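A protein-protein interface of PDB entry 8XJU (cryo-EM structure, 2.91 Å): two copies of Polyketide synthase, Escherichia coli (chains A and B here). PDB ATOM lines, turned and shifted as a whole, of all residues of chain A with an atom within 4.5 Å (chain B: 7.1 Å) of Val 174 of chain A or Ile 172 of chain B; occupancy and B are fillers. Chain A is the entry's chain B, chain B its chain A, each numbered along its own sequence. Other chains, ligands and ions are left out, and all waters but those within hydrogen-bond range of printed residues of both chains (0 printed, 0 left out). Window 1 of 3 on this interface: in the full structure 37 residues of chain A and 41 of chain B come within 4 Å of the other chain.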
ATOM      1  N   ALA A 121     -12.426 -24.118   4.564  1.00  0.00           N
ATOM      2  CA  ALA A 121     -13.766 -23.590   4.631  1.00  0.00           C
ATOM      3  C   ALA A 121     -13.899 -22.737   5.876  1.00  0.00           C
ATOM      4  O   ALA A 121     -12.984 -22.630   6.681  1.00  0.00           O
ATOM      5  CB  ALA A 121     -14.804 -24.714   4.599  1.00  0.00           C
ATOM      6  N   GLY A 122     -15.048 -22.102   6.010  1.00  0.00           N
ATOM      7  CA  GLY A 122     -15.353 -21.351   7.200  1.00  0.00           C
ATOM      8  C   GLY A 122     -16.786 -21.588   7.609  1.00  0.00           C
ATOM      9  O   GLY A 122     -17.548 -22.247   6.921  1.00  0.00           O
ATOM     10  N   ILE A 172      -8.044 -26.762   6.810  1.00  0.00           N
ATOM     11  CA  ILE A 172      -7.814 -25.516   7.527  1.00  0.00           C
ATOM     12  C   ILE A 172      -9.108 -24.721   7.566  1.00  0.00           C
ATOM     13  O   ILE A 172      -9.606 -24.293   6.524  1.00  0.00           O
ATOM     14  CB  ILE A 172      -6.694 -24.706   6.866  1.00  0.00           C
ATOM     15  CG1 ILE A 172      -5.404 -25.521   6.857  1.00  0.00           C
ATOM     16  CG2 ILE A 172      -6.515 -23.384   7.573  1.00  0.00           C
ATOM     17  CD1 ILE A 172      -4.296 -24.905   6.080  1.00  0.00           C
ATOM     18  N   THR A 173      -9.653 -24.519   8.759  1.00  0.00           N
ATOM     19  CA  THR A 173     -10.765 -23.595   8.932  1.00  0.00           C
ATOM     20  C   THR A 173     -10.233 -22.167   8.971  1.00  0.00           C
ATOM     21  O   THR A 173      -9.343 -21.855   9.762  1.00  0.00           O
ATOM     22  CB  THR A 173     -11.523 -23.900  10.219  1.00  0.00           C
ATOM     23  OG1 THR A 173     -12.236 -25.118  10.084  1.00  0.00           O
ATOM     24  CG2 THR A 173     -12.518 -22.831  10.526  1.00  0.00           C
ATOM     25  N   VAL A 174     -10.755 -21.303   8.107  1.00  0.00           N
ATOM     26  CA  VAL A 174     -10.439 -19.881   8.138  1.00  0.00           C
ATOM     27  C   VAL A 174     -11.663 -19.156   8.684  1.00  0.00           C
ATOM     28  O   VAL A 174     -12.789 -19.637   8.541  1.00  0.00           O
ATOM     29  CB  VAL A 174     -10.018 -19.354   6.754  1.00  0.00           C
ATOM     30  CG1 VAL A 174      -8.945 -20.237   6.159  1.00  0.00           C
ATOM     31  CG2 VAL A 174     -11.162 -19.297   5.848  1.00  0.00           C
ATOM     32  N   GLN A 175     -11.442 -18.073   9.417  1.00  0.00           N
ATOM     33  CA  GLN A 175     -12.550 -17.447  10.127  1.00  0.00           C
ATOM     34  C   GLN A 175     -12.471 -15.927  10.091  1.00  0.00           C
ATOM     35  O   GLN A 175     -12.539 -15.268  11.127  1.00  0.00           O
ATOM     36  CB  GLN A 175     -12.644 -17.935  11.570  1.00  0.00           C
ATOM     37  CG  GLN A 175     -13.369 -19.263  11.757  1.00  0.00           C
ATOM     38  CD  GLN A 175     -14.813 -19.253  11.284  1.00  0.00           C
ATOM     39  OE1 GLN A 175     -15.104 -19.579  10.143  1.00  0.00           O
ATOM     40  NE2 GLN A 175     -15.728 -18.914  12.182  1.00  0.00           N
ATOM     41  N   THR A 176     -12.339 -15.327   8.907  1.00  0.00           N
ATOM     42  CA  THR A 176     -12.620 -13.894   8.834  1.00  0.00           C
ATOM     43  C   THR A 176     -14.139 -13.692   8.879  1.00  0.00           C
ATOM     44  O   THR A 176     -14.904 -14.650   8.948  1.00  0.00           O
ATOM     45  CB  THR A 176     -11.978 -13.265   7.603  1.00  0.00           C
ATOM     46  OG1 THR A 176     -12.721 -13.612   6.449  1.00  0.00           O
ATOM     47  CG2 THR A 176     -10.576 -13.804   7.413  1.00  0.00           C
ATOM     48  N   THR A 180     -15.152 -14.641   4.616  1.00  0.00           N
ATOM     49  CA  THR A 180     -14.600 -15.911   5.068  1.00  0.00           C
ATOM     50  C   THR A 180     -14.418 -16.858   3.902  1.00  0.00           C
ATOM     51  O   THR A 180     -13.367 -17.482   3.743  1.00  0.00           O
ATOM     52  CB  THR A 180     -15.538 -16.551   6.072  1.00  0.00           C
ATOM     53  OG1 THR A 180     -15.722 -15.690   7.177  1.00  0.00           O
ATOM     54  CG2 THR A 180     -14.933 -17.795   6.589  1.00  0.00           C
ATOM     55  N   VAL A 183     -11.806 -15.538   1.295  1.00  0.00           N
ATOM     56  CA  VAL A 183     -10.492 -15.706   1.906  1.00  0.00           C
ATOM     57  C   VAL A 183     -10.113 -17.178   1.952  1.00  0.00           C
ATOM     58  O   VAL A 183      -8.954 -17.537   1.734  1.00  0.00           O
ATOM     59  CB  VAL A 183     -10.478 -15.037   3.295  1.00  0.00           C
ATOM     60  CG1 VAL A 183      -9.338 -15.526   4.161  1.00  0.00           C
ATOM     61  CG2 VAL A 183     -10.327 -13.554   3.129  1.00  0.00           C
ATOM     62  N   ALA A 184     -11.096 -18.052   2.190  1.00  0.00           N
ATOM     63  CA  ALA A 184     -10.918 -19.497   2.114  1.00  0.00           C
ATOM     64  C   ALA A 184     -10.489 -19.932   0.727  1.00  0.00           C
ATOM     65  O   ALA A 184      -9.592 -20.763   0.573  1.00  0.00           O
ATOM     66  CB  ALA A 184     -12.225 -20.173   2.492  1.00  0.00           C
ATOM     67  N   VAL A 187      -6.838 -18.719   0.332  1.00  0.00           N
ATOM     68  CA  VAL A 187      -5.951 -19.604   1.085  1.00  0.00           C
ATOM     69  C   VAL A 187      -5.780 -20.934   0.357  1.00  0.00           C
ATOM     70  O   VAL A 187      -4.667 -21.469   0.264  1.00  0.00           O
ATOM     71  CB  VAL A 187      -6.503 -19.784   2.515  1.00  0.00           C
ATOM     72  CG1 VAL A 187      -5.893 -20.977   3.214  1.00  0.00           C
ATOM     73  CG2 VAL A 187      -6.254 -18.548   3.328  1.00  0.00           C
ATOM     74  N   GLY B 118       0.856  -9.293   7.927  1.00  0.00           N
ATOM     75  CA  GLY B 118      -0.254 -10.173   8.225  1.00  0.00           C
ATOM     76  C   GLY B 118      -0.231 -10.800   9.607  1.00  0.00           C
ATOM     77  O   GLY B 118       0.814 -11.090  10.152  1.00  0.00           O
ATOM     78  N   ILE B 119      -1.420 -10.996  10.152  1.00  0.00           N
ATOM     79  CA  ILE B 119      -1.698 -11.793  11.345  1.00  0.00           C
ATOM     80  C   ILE B 119      -2.451 -13.056  10.947  1.00  0.00           C
ATOM     81  O   ILE B 119      -3.451 -13.009  10.225  1.00  0.00           O
ATOM     82  CB  ILE B 119      -2.440 -10.960  12.419  1.00  0.00           C
ATOM     83  CG1 ILE B 119      -2.591 -11.633  13.804  1.00  0.00           C
ATOM     84  CG2 ILE B 119      -3.631 -10.244  11.904  1.00  0.00           C
ATOM     85  CD1 ILE B 119      -1.446 -11.908  14.607  1.00  0.00           C
ATOM     86  N   PHE B 120      -1.933 -14.194  11.393  1.00  0.00           N
ATOM     87  CA  PHE B 120      -2.512 -15.510  11.149  1.00  0.00           C
ATOM     88  C   PHE B 120      -2.494 -16.203  12.496  1.00  0.00           C
ATOM     89  O   PHE B 120      -1.471 -16.750  12.877  1.00  0.00           O
ATOM     90  CB  PHE B 120      -1.705 -16.304  10.134  1.00  0.00           C
ATOM     91  CG  PHE B 120      -1.505 -15.613   8.829  1.00  0.00           C
ATOM     92  CD1 PHE B 120      -0.432 -14.769   8.629  1.00  0.00           C
ATOM     93  CD2 PHE B 120      -2.373 -15.826   7.785  1.00  0.00           C
ATOM     94  CE1 PHE B 120      -0.239 -14.153   7.426  1.00  0.00           C
ATOM     95  CE2 PHE B 120      -2.174 -15.204   6.583  1.00  0.00           C
ATOM     96  CZ  PHE B 120      -1.111 -14.370   6.414  1.00  0.00           C
ATOM     97  N   ALA B 121      -3.575 -16.175  13.244  1.00  0.00           N
ATOM     98  CA  ALA B 121      -3.508 -16.718  14.581  1.00  0.00           C
ATOM     99  C   ALA B 121      -4.742 -17.553  14.846  1.00  0.00           C
ATOM    100  O   ALA B 121      -5.667 -17.601  14.046  1.00  0.00           O
ATOM    101  CB  ALA B 121      -3.349 -15.605  15.619  1.00  0.00           C
ATOM    102  N   GLY B 122      -4.743 -18.222  15.985  1.00  0.00           N
ATOM    103  CA  GLY B 122      -5.880 -18.991  16.416  1.00  0.00           C
ATOM    104  C   GLY B 122      -6.187 -18.748  17.870  1.00  0.00           C
ATOM    105  O   GLY B 122      -5.555 -17.920  18.516  1.00  0.00           O
ATOM    106  N   SER B 156     -13.424 -10.829  16.040  1.00  0.00           N
ATOM    107  CA  SER B 156     -12.433 -11.858  15.730  1.00  0.00           C
ATOM    108  C   SER B 156     -11.015 -11.406  16.044  1.00  0.00           C
ATOM    109  O   SER B 156     -10.665 -10.235  15.894  1.00  0.00           O
ATOM    110  CB  SER B 156     -12.519 -12.246  14.258  1.00  0.00           C
ATOM    111  OG  SER B 156     -11.532 -13.198  13.920  1.00  0.00           O
ATOM    112  N   ILE B 157     -10.197 -12.374  16.463  1.00  0.00           N
ATOM    113  CA  ILE B 157      -8.958 -12.114  17.189  1.00  0.00           C
ATOM    114  C   ILE B 157      -7.892 -11.486  16.298  1.00  0.00           C
ATOM    115  O   ILE B 157      -7.209 -10.538  16.710  1.00  0.00           O
ATOM    116  CB  ILE B 157      -8.512 -13.427  17.884  1.00  0.00           C
ATOM    117  CG1 ILE B 157      -7.372 -13.210  18.872  1.00  0.00           C
ATOM    118  CG2 ILE B 157      -8.200 -14.587  16.915  1.00  0.00           C
ATOM    119  CD1 ILE B 157      -7.202 -14.383  19.744  1.00  0.00           C
ATOM    120  N   THR B 158      -7.766 -11.950  15.062  1.00  0.00           N
ATOM    121  CA  THR B 158      -6.783 -11.412  14.146  1.00  0.00           C
ATOM    122  C   THR B 158      -7.146 -10.025  13.664  1.00  0.00           C
ATOM    123  O   THR B 158      -6.257  -9.202  13.483  1.00  0.00           O
ATOM    124  CB  THR B 158      -6.614 -12.346  12.957  1.00  0.00           C
ATOM    125  OG1 THR B 158      -7.903 -12.787  12.524  1.00  0.00           O
ATOM    126  CG2 THR B 158      -5.778 -13.520  13.335  1.00  0.00           C
ATOM    127  N   THR B 159      -8.426  -9.733  13.485  1.00  0.00           N
ATOM    128  CA  THR B 159      -8.824  -8.392  13.100  1.00  0.00           C
ATOM    129  C   THR B 159      -8.789  -7.412  14.261  1.00  0.00           C
ATOM    130  O   THR B 159      -8.544  -6.228  14.031  1.00  0.00           O
ATOM    131  CB  THR B 159     -10.211  -8.409  12.465  1.00  0.00           C
ATOM    132  OG1 THR B 159     -11.172  -8.903  13.403  1.00  0.00           O
ATOM    133  CG2 THR B 159     -10.206  -9.283  11.238  1.00  0.00           C
ATOM    134  N   GLY B 169      -1.876  -6.406   6.078  1.00  0.00           N
ATOM    135  CA  GLY B 169      -1.816  -7.600   5.281  1.00  0.00           C
ATOM    136  C   GLY B 169      -2.944  -8.492   5.734  1.00  0.00           C
ATOM    137  O   GLY B 169      -3.816  -8.052   6.481  1.00  0.00           O
ATOM    138  N   PRO B 170      -2.937  -9.758   5.318  1.00  0.00           N
ATOM    139  CA  PRO B 170      -4.075 -10.648   5.591  1.00  0.00           C
ATOM    140  C   PRO B 170      -4.250 -10.953   7.072  1.00  0.00           C
ATOM    141  O   PRO B 170      -3.312 -11.372   7.744  1.00  0.00           O
ATOM    142  CB  PRO B 170      -3.721 -11.913   4.807  1.00  0.00           C
ATOM    143  CG  PRO B 170      -2.658 -11.530   3.874  1.00  0.00           C
ATOM    144  CD  PRO B 170      -1.927 -10.402   4.468  1.00  0.00           C
ATOM    145  N   ALA B 171      -5.467 -10.768   7.571  1.00  0.00           N
ATOM    146  CA  ALA B 171      -5.812 -11.055   8.963  1.00  0.00           C
ATOM    147  C   ALA B 171      -6.753 -12.259   9.014  1.00  0.00           C
ATOM    148  O   ALA B 171      -7.971 -12.108   9.108  1.00  0.00           O
ATOM    149  CB  ALA B 171      -6.449  -9.850   9.623  1.00  0.00           C
ATOM    150  N   ILE B 172      -6.178 -13.456   9.011  1.00  0.00           N
ATOM    151  CA  ILE B 172      -6.922 -14.698   8.843  1.00  0.00           C
ATOM    152  C   ILE B 172      -6.855 -15.492  10.140  1.00  0.00           C
ATOM    153  O   ILE B 172      -5.768 -15.849  10.596  1.00  0.00           O
ATOM    154  CB  ILE B 172      -6.371 -15.509   7.662  1.00  0.00           C
ATOM    155  CG1 ILE B 172      -6.310 -14.626   6.417  1.00  0.00           C
ATOM    156  CG2 ILE B 172      -7.219 -16.737   7.413  1.00  0.00           C
ATOM    157  CD1 ILE B 172      -5.542 -15.196   5.281  1.00  0.00           C
ATOM    158  N   THR B 173      -8.011 -15.780  10.731  1.00  0.00           N
ATOM    159  CA  THR B 173      -8.072 -16.630  11.916  1.00  0.00           C
ATOM    160  C   THR B 173      -8.048 -18.088  11.472  1.00  0.00           C
ATOM    161  O   THR B 173      -9.077 -18.740  11.293  1.00  0.00           O
ATOM    162  CB  THR B 173      -9.305 -16.333  12.753  1.00  0.00           C
ATOM    163  OG1 THR B 173      -9.455 -14.924  12.913  1.00  0.00           O
ATOM    164  CG2 THR B 173      -9.171 -16.950  14.112  1.00  0.00           C
ATOM    165  N   VAL B 174      -6.827 -18.589  11.272  1.00  0.00           N
ATOM    166  CA  VAL B 174      -6.580 -20.007  11.061  1.00  0.00           C
ATOM    167  C   VAL B 174      -7.000 -20.788  12.295  1.00  0.00           C
ATOM    168  O   VAL B 174      -6.604 -20.445  13.409  1.00  0.00           O
ATOM    169  CB  VAL B 174      -5.091 -20.210  10.767  1.00  0.00           C
ATOM    170  CG1 VAL B 174      -4.724 -21.662  10.875  1.00  0.00           C
ATOM    171  CG2 VAL B 174      -4.739 -19.648   9.417  1.00  0.00           C
ATOM    172  N   GLN B 175      -7.840 -21.822  12.117  1.00  0.00           N
ATOM    173  CA  GLN B 175      -8.323 -22.617  13.259  1.00  0.00           C
ATOM    174  C   GLN B 175      -8.390 -24.117  12.955  1.00  0.00           C
ATOM    175  O   GLN B 175      -9.456 -24.636  12.637  1.00  0.00           O
ATOM    176  CB  GLN B 175      -9.686 -22.123  13.725  1.00  0.00           C
ATOM    177  CG  GLN B 175      -9.700 -20.768  14.402  1.00  0.00           C
ATOM    178  CD  GLN B 175      -9.517 -20.839  15.896  1.00  0.00           C
ATOM    179  OE1 GLN B 175      -8.657 -21.552  16.392  1.00  0.00           O
ATOM    180  NE2 GLN B 175     -10.335 -20.092  16.622  1.00  0.00           N
ATOM    181  N   THR B 176      -7.285 -24.830  13.158  1.00  0.00           N
ATOM    182  CA  THR B 176      -7.369 -26.273  13.353  1.00  0.00           C
ATOM    183  C   THR B 176      -7.475 -26.529  14.861  1.00  0.00           C
ATOM    184  O   THR B 176      -7.757 -25.610  15.630  1.00  0.00           O
ATOM    185  CB  THR B 176      -6.221 -26.986  12.641  1.00  0.00           C
ATOM    186  OG1 THR B 176      -4.978 -26.384  12.963  1.00  0.00           O
ATOM    187  CG2 THR B 176      -6.403 -26.863  11.157  1.00  0.00           C
ATOM    188  N   ALA B 184      -1.054 -22.076  11.511  1.00  0.00           N
ATOM    189  CA  ALA B 184      -1.044 -20.630  11.319  1.00  0.00           C
ATOM    190  C   ALA B 184       0.320 -20.134  10.875  1.00  0.00           C
ATOM    191  O   ALA B 184       0.412 -19.253  10.022  1.00  0.00           O
ATOM    192  CB  ALA B 184      -1.473 -19.959  12.613  1.00  0.00           C
ATOM    193  N   VAL B 187       0.477 -21.234   7.178  1.00  0.00           N
ATOM    194  CA  VAL B 187      -0.310 -20.332   6.339  1.00  0.00           C
ATOM    195  C   VAL B 187       0.396 -18.990   6.186  1.00  0.00           C
ATOM    196  O   VAL B 187       0.413 -18.396   5.098  1.00  0.00           O
ATOM    197  CB  VAL B 187      -1.722 -20.176   6.930  1.00  0.00           C
ATOM    198  CG1 VAL B 187      -2.521 -19.144   6.182  1.00  0.00           C
ATOM    199  CG2 VAL B 187      -2.447 -21.476   6.877  1.00  0.00           C
ATOM    200  N   SER B 191       1.727 -17.195   2.738  1.00  0.00           N
ATOM    201  CA  SER B 191       1.518 -15.791   2.379  1.00  0.00           C
ATOM    202  C   SER B 191       2.825 -15.061   2.133  1.00  0.00           C
ATOM    203  O   SER B 191       2.904 -14.195   1.263  1.00  0.00           O
ATOM    204  CB  SER B 191       0.743 -15.076   3.469  1.00  0.00           C
ATOM    205  OG  SER B 191      -0.634 -15.336   3.365  1.00  0.00           O
ATOM    206  N   GLN B 196       2.120 -12.437  -0.597  1.00  0.00           N
ATOM    207  CA  GLN B 196       0.892 -11.812  -0.125  1.00  0.00           C
ATOM    208  C   GLN B 196       1.159 -10.792   0.964  1.00  0.00           C
ATOM    209  O   GLN B 196       0.325  -9.913   1.193  1.00  0.00           O
ATOM    210  CB  GLN B 196      -0.076 -12.856   0.421  1.00  0.00           C
ATOM    211  CG  GLN B 196      -0.912 -13.551  -0.610  1.00  0.00           C
ATOM    212  CD  GLN B 196      -2.202 -12.830  -0.904  1.00  0.00           C
ATOM    213  OE1 GLN B 196      -2.387 -12.284  -1.986  1.00  0.00           O
ATOM    214  NE2 GLN B 196      -3.105 -12.831   0.058  1.00  0.00           N
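O of Thr 173 of chain A sits at hydrogen-bond distance from N of Gln 175 of chain B, 2.8 Å away. The backbone carbonyl oxygen of Thr 173 of chain B sits close to the backbone carbonyl oxygen of Thr 173 of chain A (3.5 Å). The backbone carbonyl oxygen (O) of Thr 173 of chain B sits at hydrogen-bond distance from the backbone NH (N) of Gln 175 of chain A (3.1 Å).
Ile 172 of chain A touches Val 187 of chain B, and with the chains exchanged Val 187 of chain A touches Ile 172 of chain B. Thr 173 of chain A touches Val 174 of chain B, and with the chains exchanged Val 174 of chain A touches Thr 173 of chain B. Thr 173 of chain A touches Gln 175 of chain B, and with the chains exchanged Gln 175 of chain A touches Thr 173 of chain B. Val 174 of chain A touches Ile 172 of chain B, but with the chains exchanged Ile 172 of chain A does not touch Val 174 of chain B (4.1 Å). 9 positions are printed for both chains. Of the 11 pairs that touch across the chains among the printed residues, 7 have their exchanged pair printed and touching as well.
Ile 172 of chain A touches Val 187 of chain B (CD1 to CG2, 3.98 Å). Val 174 of chain B touches Thr 173 of chain A. Ile 172 of chain B touches Val 174 of chain A. CA of Val 174 of chain A touches O of Thr 173 of chain B, 3.6 Å away. O of Gln 175 of chain A touches OG of Ser 156 of chain B (3.6 Å). Ala 171 of chain B touches Thr 176 of chain A (O to CG2, 3.5 Å). Ile 172 of chain B touches Val 183 of chain A (CG1 to CG1, 3.9 Å). CG2 of Val 187 of chain A touches CD1 of Ile 172 of chain B (3.9 Å).
Printed residues of chain B within 4 Å of Ile 172 of chain A: Val 187. Of the printed residues of chain B, Thr 173 of chain A touches Thr 173 (3.5 Å), Val 174 (3.6 Å) and Gln 175 (2.8 Å). Of the printed residues of chain B, Gln 175 of chain A touches Ser 156 (3.6 Å) and Thr 173 (3.1 Å). Of the printed residues of chain A, Ser 156 of chain B touches Gln 175 (3.6 Å). Printed residues of chain A within 4 Å of Val 187 of chain B: Ile 172 (3.98 Å). The nearest residue of chain A that does not touch Ile 172 of chain B is Thr 176 of chain A (4.02 Å).
Of the 21 printed residues of chain B, 7 touch a printed residue of chain A. Hydrophobic or aromatic side chains of chain B within 4 Å of the printed part of chain A: Ile 172 and Val 187. Of the 11 printed residues of chain A, 7 touch a printed residue of chain B. Hydrophobic or aromatic side chains of chain A that line the printed part of chain B: Ile 172, Val 174, Val 183 and Val 187. Among the printed residues, 11 pairs touch across the chains. Among the printed residues, no Asp or Glu carboxylate lies within 4 Å of a Lys or Arg side-chain nitrogen of the other chain.
The backbone NH (N) of Ala 121 of chain A is in hydrogen-bond range of the backbone carbonyl oxygen (O) of Ile 172 of chain A (3.4 Å). OG of Ser 156 of chain B is in hydrogen-bond range of OG1 of Thr 173 of chain B. The backbone NH (N) of Ala 121 of chain B sits at hydrogen-bond distance from the backbone carbonyl oxygen (O) of Ile 172 of chain B, 3.5 Å away. O of Ala 121 of chain A sits at hydrogen-bond distance from N of Val 174 of chain A (3.0 Å). The side-chain hydroxyl (OG1) of Thr 159 of chain B sits at hydrogen-bond distance from the backbone carbonyl oxygen (O) of Ser 156 of chain B (2.9 Å). The backbone carbonyl oxygen (O) of Ala 121 of chain B is in hydrogen-bond range of the backbone NH (N) of Val 174 of chain B, 3.2 Å away.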
